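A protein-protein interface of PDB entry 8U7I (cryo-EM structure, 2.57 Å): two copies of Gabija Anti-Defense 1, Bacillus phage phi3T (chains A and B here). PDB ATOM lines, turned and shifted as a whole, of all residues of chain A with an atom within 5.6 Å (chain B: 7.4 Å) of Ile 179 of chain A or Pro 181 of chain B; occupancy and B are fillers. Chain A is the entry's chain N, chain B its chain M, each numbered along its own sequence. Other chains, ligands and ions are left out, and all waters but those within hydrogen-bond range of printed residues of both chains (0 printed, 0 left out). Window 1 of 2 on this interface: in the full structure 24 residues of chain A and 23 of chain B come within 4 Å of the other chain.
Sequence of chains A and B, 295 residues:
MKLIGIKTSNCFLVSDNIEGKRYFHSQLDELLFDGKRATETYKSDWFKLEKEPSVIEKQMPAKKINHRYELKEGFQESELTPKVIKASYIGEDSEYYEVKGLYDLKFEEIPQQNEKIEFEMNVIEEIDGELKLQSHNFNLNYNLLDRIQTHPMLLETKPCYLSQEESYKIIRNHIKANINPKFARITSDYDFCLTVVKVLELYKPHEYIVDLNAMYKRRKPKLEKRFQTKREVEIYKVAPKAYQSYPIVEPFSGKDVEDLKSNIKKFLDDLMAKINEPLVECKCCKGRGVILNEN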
ATOM      1  N   HIS A 174       5.489   5.563  11.662  1.00  0.00           N
ATOM      2  CA  HIS A 174       5.815   6.397  12.813  1.00  0.00           C
ATOM      3  C   HIS A 174       4.736   6.328  13.883  1.00  0.00           C
ATOM      4  O   HIS A 174       5.053   6.331  15.078  1.00  0.00           O
ATOM      5  CB  HIS A 174       6.028   7.845  12.384  1.00  0.00           C
ATOM      6  CG  HIS A 174       6.868   8.630  13.341  1.00  0.00           C
ATOM      7  ND1 HIS A 174       6.329   9.386  14.359  1.00  0.00           N
ATOM      8  CD2 HIS A 174       8.211   8.770  13.439  1.00  0.00           C
ATOM      9  CE1 HIS A 174       7.302   9.956  15.044  1.00  0.00           C
ATOM     10  NE2 HIS A 174       8.454   9.602  14.504  1.00  0.00           N
ATOM     11  N   ILE A 175       3.465   6.279  13.481  1.00  0.00           N
ATOM     12  CA  ILE A 175       2.386   6.150  14.456  1.00  0.00           C
ATOM     13  C   ILE A 175       2.545   4.854  15.236  1.00  0.00           C
ATOM     14  O   ILE A 175       2.445   4.828  16.468  1.00  0.00           O
ATOM     15  CB  ILE A 175       1.019   6.224  13.757  1.00  0.00           C
ATOM     16  CG1 ILE A 175       0.677   7.672  13.419  1.00  0.00           C
ATOM     17  CG2 ILE A 175      -0.060   5.625  14.634  1.00  0.00           C
ATOM     18  CD1 ILE A 175      -0.721   7.851  12.899  1.00  0.00           C
ATOM     19  N   LYS A 176       2.834   3.761  14.532  1.00  0.00           N
ATOM     20  CA  LYS A 176       3.092   2.499  15.210  1.00  0.00           C
ATOM     21  C   LYS A 176       4.328   2.579  16.091  1.00  0.00           C
ATOM     22  O   LYS A 176       4.521   1.732  16.968  1.00  0.00           O
ATOM     23  CB  LYS A 176       3.248   1.380  14.182  1.00  0.00           C
ATOM     24  CG  LYS A 176       2.701   0.042  14.633  1.00  0.00           C
ATOM     25  CD  LYS A 176       2.975  -1.035  13.601  1.00  0.00           C
ATOM     26  CE  LYS A 176       2.567  -0.581  12.213  1.00  0.00           C
ATOM     27  NZ  LYS A 176       2.728  -1.673  11.216  1.00  0.00           N
ATOM     28  N   ALA A 177       5.175   3.588  15.878  1.00  0.00           N
ATOM     29  CA  ALA A 177       6.485   3.599  16.519  1.00  0.00           C
ATOM     30  C   ALA A 177       6.439   4.238  17.902  1.00  0.00           C
ATOM     31  O   ALA A 177       6.992   3.692  18.863  1.00  0.00           O
ATOM     32  CB  ALA A 177       7.497   4.319  15.630  1.00  0.00           C
ATOM     33  N   ASN A 178       5.808   5.404  18.026  1.00  0.00           N
ATOM     34  CA  ASN A 178       5.984   6.216  19.225  1.00  0.00           C
ATOM     35  C   ASN A 178       4.662   6.730  19.778  1.00  0.00           C
ATOM     36  O   ASN A 178       4.593   7.834  20.324  1.00  0.00           O
ATOM     37  CB  ASN A 178       6.929   7.384  18.950  1.00  0.00           C
ATOM     38  CG  ASN A 178       7.933   7.075  17.861  1.00  0.00           C
ATOM     39  OD1 ASN A 178       7.860   7.620  16.761  1.00  0.00           O
ATOM     40  ND2 ASN A 178       8.881   6.199  18.163  1.00  0.00           N
ATOM     41  N   ILE A 179       3.591   5.958  19.664  1.00  0.00           N
ATOM     42  CA  ILE A 179       2.358   6.326  20.344  1.00  0.00           C
ATOM     43  C   ILE A 179       2.427   5.869  21.794  1.00  0.00           C
ATOM     44  O   ILE A 179       3.253   5.034  22.173  1.00  0.00           O
ATOM     45  CB  ILE A 179       1.086   5.811  19.615  1.00  0.00           C
ATOM     46  CG1 ILE A 179       1.049   4.283  19.371  1.00  0.00           C
ATOM     47  CG2 ILE A 179       0.841   6.607  18.341  1.00  0.00           C
ATOM     48  CD1 ILE A 179       1.153   3.348  20.559  1.00  0.00           C
ATOM     49  N   ASN A 180       1.570   6.451  22.624  1.00  0.00           N
ATOM     50  CA  ASN A 180       1.553   6.124  24.037  1.00  0.00           C
ATOM     51  C   ASN A 180       0.352   5.244  24.333  1.00  0.00           C
ATOM     52  O   ASN A 180      -0.791   5.699  24.182  1.00  0.00           O
ATOM     53  CB  ASN A 180       1.511   7.391  24.886  1.00  0.00           C
ATOM     54  CG  ASN A 180       2.398   7.296  26.107  1.00  0.00           C
ATOM     55  OD1 ASN A 180       3.210   6.380  26.226  1.00  0.00           O
ATOM     56  ND2 ASN A 180       2.249   8.245  27.022  1.00  0.00           N
ATOM     57  N   PRO A 181       0.556   3.991  24.739  1.00  0.00           N
ATOM     58  CA  PRO A 181      -0.591   3.141  25.092  1.00  0.00           C
ATOM     59  C   PRO A 181      -1.400   3.683  26.251  1.00  0.00           C
ATOM     60  O   PRO A 181      -2.561   3.288  26.416  1.00  0.00           O
ATOM     61  CB  PRO A 181       0.062   1.796  25.438  1.00  0.00           C
ATOM     62  CG  PRO A 181       1.395   1.837  24.770  1.00  0.00           C
ATOM     63  CD  PRO A 181       1.831   3.263  24.827  1.00  0.00           C
ATOM     64  N   ALA A 184      -3.416   6.378  23.787  1.00  0.00           N
ATOM     65  CA  ALA A 184      -3.949   6.031  22.478  1.00  0.00           C
ATOM     66  C   ALA A 184      -3.722   4.554  22.197  1.00  0.00           C
ATOM     67  O   ALA A 184      -2.808   3.929  22.740  1.00  0.00           O
ATOM     68  CB  ALA A 184      -3.319   6.885  21.373  1.00  0.00           C
ATOM     69  N   ILE A 186      -4.222   1.537  18.754  1.00  0.00           N
ATOM     70  CA  ILE A 186      -4.431   1.298  17.331  1.00  0.00           C
ATOM     71  C   ILE A 186      -5.361   0.102  17.203  1.00  0.00           C
ATOM     72  O   ILE A 186      -5.045  -0.995  17.680  1.00  0.00           O
ATOM     73  CB  ILE A 186      -3.112   1.053  16.591  1.00  0.00           C
ATOM     74  CG1 ILE A 186      -2.100   2.149  16.923  1.00  0.00           C
ATOM     75  CG2 ILE A 186      -3.352   0.985  15.095  1.00  0.00           C
ATOM     76  CD1 ILE A 186      -0.799   2.018  16.170  1.00  0.00           C
ATOM     77  N   VAL A 196      -6.516   4.683  14.485  1.00  0.00           N
ATOM     78  CA  VAL A 196      -6.024   4.797  15.850  1.00  0.00           C
ATOM     79  C   VAL A 196      -7.074   5.550  16.650  1.00  0.00           C
ATOM     80  O   VAL A 196      -7.567   6.591  16.205  1.00  0.00           O
ATOM     81  CB  VAL A 196      -4.661   5.511  15.905  1.00  0.00           C
ATOM     82  CG1 VAL A 196      -4.593   6.600  14.854  1.00  0.00           C
ATOM     83  CG2 VAL A 196      -4.405   6.078  17.288  1.00  0.00           C
ATOM     84  N   MET A 272       0.740  13.834  15.736  1.00  0.00           N
ATOM     85  CA  MET A 272       1.086  12.857  16.756  1.00  0.00           C
ATOM     86  C   MET A 272       0.949  13.436  18.158  1.00  0.00           C
ATOM     87  O   MET A 272       0.659  12.697  19.105  1.00  0.00           O
ATOM     88  CB  MET A 272       2.505  12.352  16.507  1.00  0.00           C
ATOM     89  CG  MET A 272       3.009  11.336  17.488  1.00  0.00           C
ATOM     90  SD  MET A 272       2.574   9.712  16.853  1.00  0.00           S
ATOM     91  CE  MET A 272       4.006   8.777  17.344  1.00  0.00           C
ATOM     92  N   ILE A 275      -2.464  13.081  19.150  1.00  0.00           N
ATOM     93  CA  ILE A 275      -2.784  11.679  19.397  1.00  0.00           C
ATOM     94  C   ILE A 275      -2.465  11.307  20.839  1.00  0.00           C
ATOM     95  O   ILE A 275      -3.261  10.653  21.521  1.00  0.00           O
ATOM     96  CB  ILE A 275      -2.034  10.779  18.399  1.00  0.00           C
ATOM     97  CG1 ILE A 275      -2.845  10.619  17.114  1.00  0.00           C
ATOM     98  CG2 ILE A 275      -1.739   9.419  19.012  1.00  0.00           C
ATOM     99  CD1 ILE A 275      -2.252   9.631  16.140  1.00  0.00           C
ATOM    100  N   ASN A 276      -1.302  11.728  21.329  1.00  0.00           N
ATOM    101  CA  ASN A 276      -0.842  11.379  22.664  1.00  0.00           C
ATOM    102  C   ASN A 276      -1.203  12.428  23.707  1.00  0.00           C
ATOM    103  O   ASN A 276      -0.774  12.315  24.859  1.00  0.00           O
ATOM    104  CB  ASN A 276       0.670  11.155  22.655  1.00  0.00           C
ATOM    105  CG  ASN A 276       1.076   9.965  21.816  1.00  0.00           C
ATOM    106  OD1 ASN A 276       0.607   8.849  22.034  1.00  0.00           O
ATOM    107  ND2 ASN A 276       1.950  10.197  20.845  1.00  0.00           N
ATOM    108  N   ASN B 178       0.886  -0.749  29.244  1.00  0.00           N
ATOM    109  CA  ASN B 178       2.181  -0.227  29.656  1.00  0.00           C
ATOM    110  C   ASN B 178       3.285  -0.481  28.639  1.00  0.00           C
ATOM    111  O   ASN B 178       4.438  -0.127  28.897  1.00  0.00           O
ATOM    112  CB  ASN B 178       2.581  -0.830  31.003  1.00  0.00           C
ATOM    113  CG  ASN B 178       1.731  -0.322  32.144  1.00  0.00           C
ATOM    114  OD1 ASN B 178       1.080   0.715  32.034  1.00  0.00           O
ATOM    115  ND2 ASN B 178       1.733  -1.053  33.251  1.00  0.00           N
ATOM    116  N   ILE B 179       2.967  -1.083  27.492  1.00  0.00           N
ATOM    117  CA  ILE B 179       4.013  -1.517  26.575  1.00  0.00           C
ATOM    118  C   ILE B 179       4.735  -0.310  25.993  1.00  0.00           C
ATOM    119  O   ILE B 179       4.157   0.769  25.811  1.00  0.00           O
ATOM    120  CB  ILE B 179       3.430  -2.414  25.466  1.00  0.00           C
ATOM    121  CG1 ILE B 179       4.547  -3.174  24.754  1.00  0.00           C
ATOM    122  CG2 ILE B 179       2.621  -1.596  24.476  1.00  0.00           C
ATOM    123  CD1 ILE B 179       4.054  -4.309  23.896  1.00  0.00           C
ATOM    124  N   ASN B 180       6.026  -0.484  25.724  1.00  0.00           N
ATOM    125  CA  ASN B 180       6.810   0.565  25.099  1.00  0.00           C
ATOM    126  C   ASN B 180       6.941   0.241  23.622  1.00  0.00           C
ATOM    127  O   ASN B 180       7.653  -0.712  23.269  1.00  0.00           O
ATOM    128  CB  ASN B 180       8.186   0.676  25.747  1.00  0.00           C
ATOM    129  CG  ASN B 180       8.845   2.014  25.489  1.00  0.00           C
ATOM    130  OD1 ASN B 180       8.450   2.751  24.586  1.00  0.00           O
ATOM    131  ND2 ASN B 180       9.855   2.339  26.285  1.00  0.00           N
ATOM    132  N   PRO B 181       6.283   0.982  22.730  1.00  0.00           N
ATOM    133  CA  PRO B 181       6.381   0.664  21.299  1.00  0.00           C
ATOM    134  C   PRO B 181       7.783   0.814  20.747  1.00  0.00           C
ATOM    135  O   PRO B 181       8.082   0.249  19.689  1.00  0.00           O
ATOM    136  CB  PRO B 181       5.410   1.660  20.649  1.00  0.00           C
ATOM    137  CG  PRO B 181       4.536   2.141  21.764  1.00  0.00           C
ATOM    138  CD  PRO B 181       5.392   2.124  22.983  1.00  0.00           C
ATOM    139  N   LYS B 182       8.654   1.557  21.429  1.00  0.00           N
ATOM    140  CA  LYS B 182      10.020   1.727  20.956  1.00  0.00           C
ATOM    141  C   LYS B 182      10.862   0.473  21.145  1.00  0.00           C
ATOM    142  O   LYS B 182      11.955   0.389  20.579  1.00  0.00           O
ATOM    143  CB  LYS B 182      10.676   2.907  21.673  1.00  0.00           C
ATOM    144  CG  LYS B 182       9.831   4.164  21.668  1.00  0.00           C
ATOM    145  CD  LYS B 182      10.544   5.313  22.353  1.00  0.00           C
ATOM    146  CE  LYS B 182      11.706   5.802  21.507  1.00  0.00           C
ATOM    147  NZ  LYS B 182      11.228   6.385  20.224  1.00  0.00           N
ATOM    148  N   PHE B 183      10.386  -0.495  21.921  1.00  0.00           N
ATOM    149  CA  PHE B 183      11.133  -1.718  22.167  1.00  0.00           C
ATOM    150  C   PHE B 183      10.377  -2.989  21.828  1.00  0.00           C
ATOM    151  O   PHE B 183      11.002  -3.954  21.387  1.00  0.00           O
ATOM    152  CB  PHE B 183      11.576  -1.789  23.635  1.00  0.00           C
ATOM    153  CG  PHE B 183      12.433  -0.637  24.060  1.00  0.00           C
ATOM    154  CD1 PHE B 183      13.681  -0.442  23.496  1.00  0.00           C
ATOM    155  CD2 PHE B 183      11.994   0.253  25.023  1.00  0.00           C
ATOM    156  CE1 PHE B 183      14.474   0.617  23.882  1.00  0.00           C
ATOM    157  CE2 PHE B 183      12.783   1.314  25.414  1.00  0.00           C
ATOM    158  CZ  PHE B 183      14.025   1.496  24.843  1.00  0.00           C
ATOM    159  N   ALA B 184       9.059  -3.022  22.004  1.00  0.00           N
ATOM    160  CA  ALA B 184       8.292  -4.233  21.761  1.00  0.00           C
ATOM    161  C   ALA B 184       7.002  -3.891  21.035  1.00  0.00           C
ATOM    162  O   ALA B 184       6.517  -2.758  21.084  1.00  0.00           O
ATOM    163  CB  ALA B 184       7.983  -4.976  23.067  1.00  0.00           C
ATOM    164  N   ARG B 185       6.452  -4.892  20.353  1.00  0.00           N
ATOM    165  CA  ARG B 185       5.202  -4.738  19.626  1.00  0.00           C
ATOM    166  C   ARG B 185       4.386  -6.013  19.759  1.00  0.00           C
ATOM    167  O   ARG B 185       4.933  -7.101  19.952  1.00  0.00           O
ATOM    168  CB  ARG B 185       5.442  -4.422  18.149  1.00  0.00           C
ATOM    169  CG  ARG B 185       5.620  -2.950  17.862  1.00  0.00           C
ATOM    170  CD  ARG B 185       6.611  -2.730  16.739  1.00  0.00           C
ATOM    171  NE  ARG B 185       7.426  -1.548  16.986  1.00  0.00           N
ATOM    172  CZ  ARG B 185       7.029  -0.308  16.744  1.00  0.00           C
ATOM    173  NH1 ARG B 185       5.845  -0.053  16.214  1.00  0.00           N
ATOM    174  NH2 ARG B 185       7.840   0.703  17.045  1.00  0.00           N
ATOM    175  N   VAL B 199      10.940  -5.657  18.890  1.00  0.00           N
ATOM    176  CA  VAL B 199      11.275  -4.964  17.649  1.00  0.00           C
ATOM    177  C   VAL B 199      12.699  -4.442  17.811  1.00  0.00           C
ATOM    178  O   VAL B 199      12.944  -3.340  18.303  1.00  0.00           O
ATOM    179  CB  VAL B 199      10.263  -3.869  17.305  1.00  0.00           C
ATOM    180  CG1 VAL B 199      10.021  -2.934  18.483  1.00  0.00           C
ATOM    181  CG2 VAL B 199      10.717  -3.095  16.078  1.00  0.00           C
ATOM    182  N   LEU B 202      15.377  -1.616  14.384  1.00  0.00           N
ATOM    183  CA  LEU B 202      16.057  -0.329  14.377  1.00  0.00           C
ATOM    184  C   LEU B 202      15.581   0.507  15.555  1.00  0.00           C
ATOM    185  O   LEU B 202      14.494   0.292  16.097  1.00  0.00           O
ATOM    186  CB  LEU B 202      15.820   0.421  13.062  1.00  0.00           C
ATOM    187  CG  LEU B 202      17.018   1.163  12.465  1.00  0.00           C
ATOM    188  CD1 LEU B 202      18.290   0.339  12.602  1.00  0.00           C
ATOM    189  CD2 LEU B 202      16.759   1.513  11.009  1.00  0.00           C
ATOM    190  N   LYS B 204      13.957   3.768  17.058  1.00  0.00           N
ATOM    191  CA  LYS B 204      12.650   4.192  16.553  1.00  0.00           C
ATOM    192  C   LYS B 204      12.487   5.629  16.049  1.00  0.00           C
ATOM    193  O   LYS B 204      11.886   5.821  14.985  1.00  0.00           O
ATOM    194  CB  LYS B 204      11.596   3.927  17.628  1.00  0.00           C
ATOM    195  CG  LYS B 204      11.143   2.481  17.646  1.00  0.00           C
ATOM    196  CD  LYS B 204      10.813   2.013  16.237  1.00  0.00           C
ATOM    197  CE  LYS B 204      10.942   0.506  16.106  1.00  0.00           C
ATOM    198  NZ  LYS B 204      10.653   0.042  14.719  1.00  0.00           N
ATOM    199  N   ASN B 276       9.956  -4.750  27.909  1.00  0.00           N
ATOM    200  CA  ASN B 276      10.303  -3.380  27.556  1.00  0.00           C
ATOM    201  C   ASN B 276      11.792  -3.087  27.675  1.00  0.00           C
ATOM    202  O   ASN B 276      12.209  -1.962  27.380  1.00  0.00           O
ATOM    203  CB  ASN B 276       9.515  -2.402  28.430  1.00  0.00           C
ATOM    204  CG  ASN B 276       8.049  -2.349  28.063  1.00  0.00           C
ATOM    205  OD1 ASN B 276       7.692  -2.306  26.885  1.00  0.00           O
ATOM    206  ND2 ASN B 276       7.186  -2.356  29.071  1.00  0.00           N
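The guanidinium group (NH2) of Arg 185 of chain B sits close to the backbone carbonyl oxygen (O) of Lys 176 of chain A, at 3.5 Å. ND2 of Asn 178 of chain A sits close to NZ of Lys 182 of chain B (3.1 Å).
The backbone carbonyl oxygen (O) of Pro 181 of chain B sits at hydrogen-bond distance from the guanidinium group (NH2) of Arg 185 of chain B, 2.7 Å away. The side-chain amide oxygen of Asn 178 of chain A lies close to a ring nitrogen (NE2) of His 174 of chain A (3.1 Å). N of Lys 182 of chain B lies close to OD1 of Asn 180 of chain B (3.4 Å).
Among the printed residues, pairs that only touch across the chains: Lys 176 of chain A with Pro 181 of chain B (3.8 Å), Ala 177 of chain A with Pro 181 of chain B (3.1 Å), Ala 177 of chain A with Lys 182 of chain B (3.7 Å), Ala 177 of chain A with Arg 185 of chain B (3.2 Å), Asn 178 of chain A with Lys 204 of chain B (3.6 Å), Ile 179 of chain A with Pro 181 of chain B (3.2 Å) and Pro 181 of chain A with Ile 179 of chain B (3.1 Å).
His 174 of chain A touches none of the printed residues of chain B. Of the printed residues of chain B, Lys 176 of chain A touches Pro 181 (3.8 Å) and Arg 185 (2.3 Å). Of the printed residues of chain B, Asn 178 of chain A touches Lys 182 and Lys 204. Of the printed residues of chain B, Ile 179 of chain A touches Pro 181. Pro 181 of chain B touches just these residues of chain A: Lys 176 (3.8 Å), Ala 177 (3.1 Å) and Ile 179 (3.2 Å). Printed residues of chain A within 4 Å of Lys 182 of chain B: Ala 177 (3.7 Å) and Asn 178 (3.1 Å). The nearest printed residue of chain B that does not touch Lys 176 of chain A is Lys 182 of chain B (6.1 Å).
Hydrophobic or aromatic side chains of chain A within 4 Å of the printed part of chain B: Ala 177, Ile 179 and Pro 181.
Ile 179 of chain A touches Pro 181 of chain B, and with the chains exchanged Pro 181 of chain A touches Ile 179 of chain B. Positions printed for both chains: 178, 179, 180, 181, 184 and 276. Of the 9 pairs that touch across the chains among the printed residues, 2 have their exchanged pair printed and touching as well.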
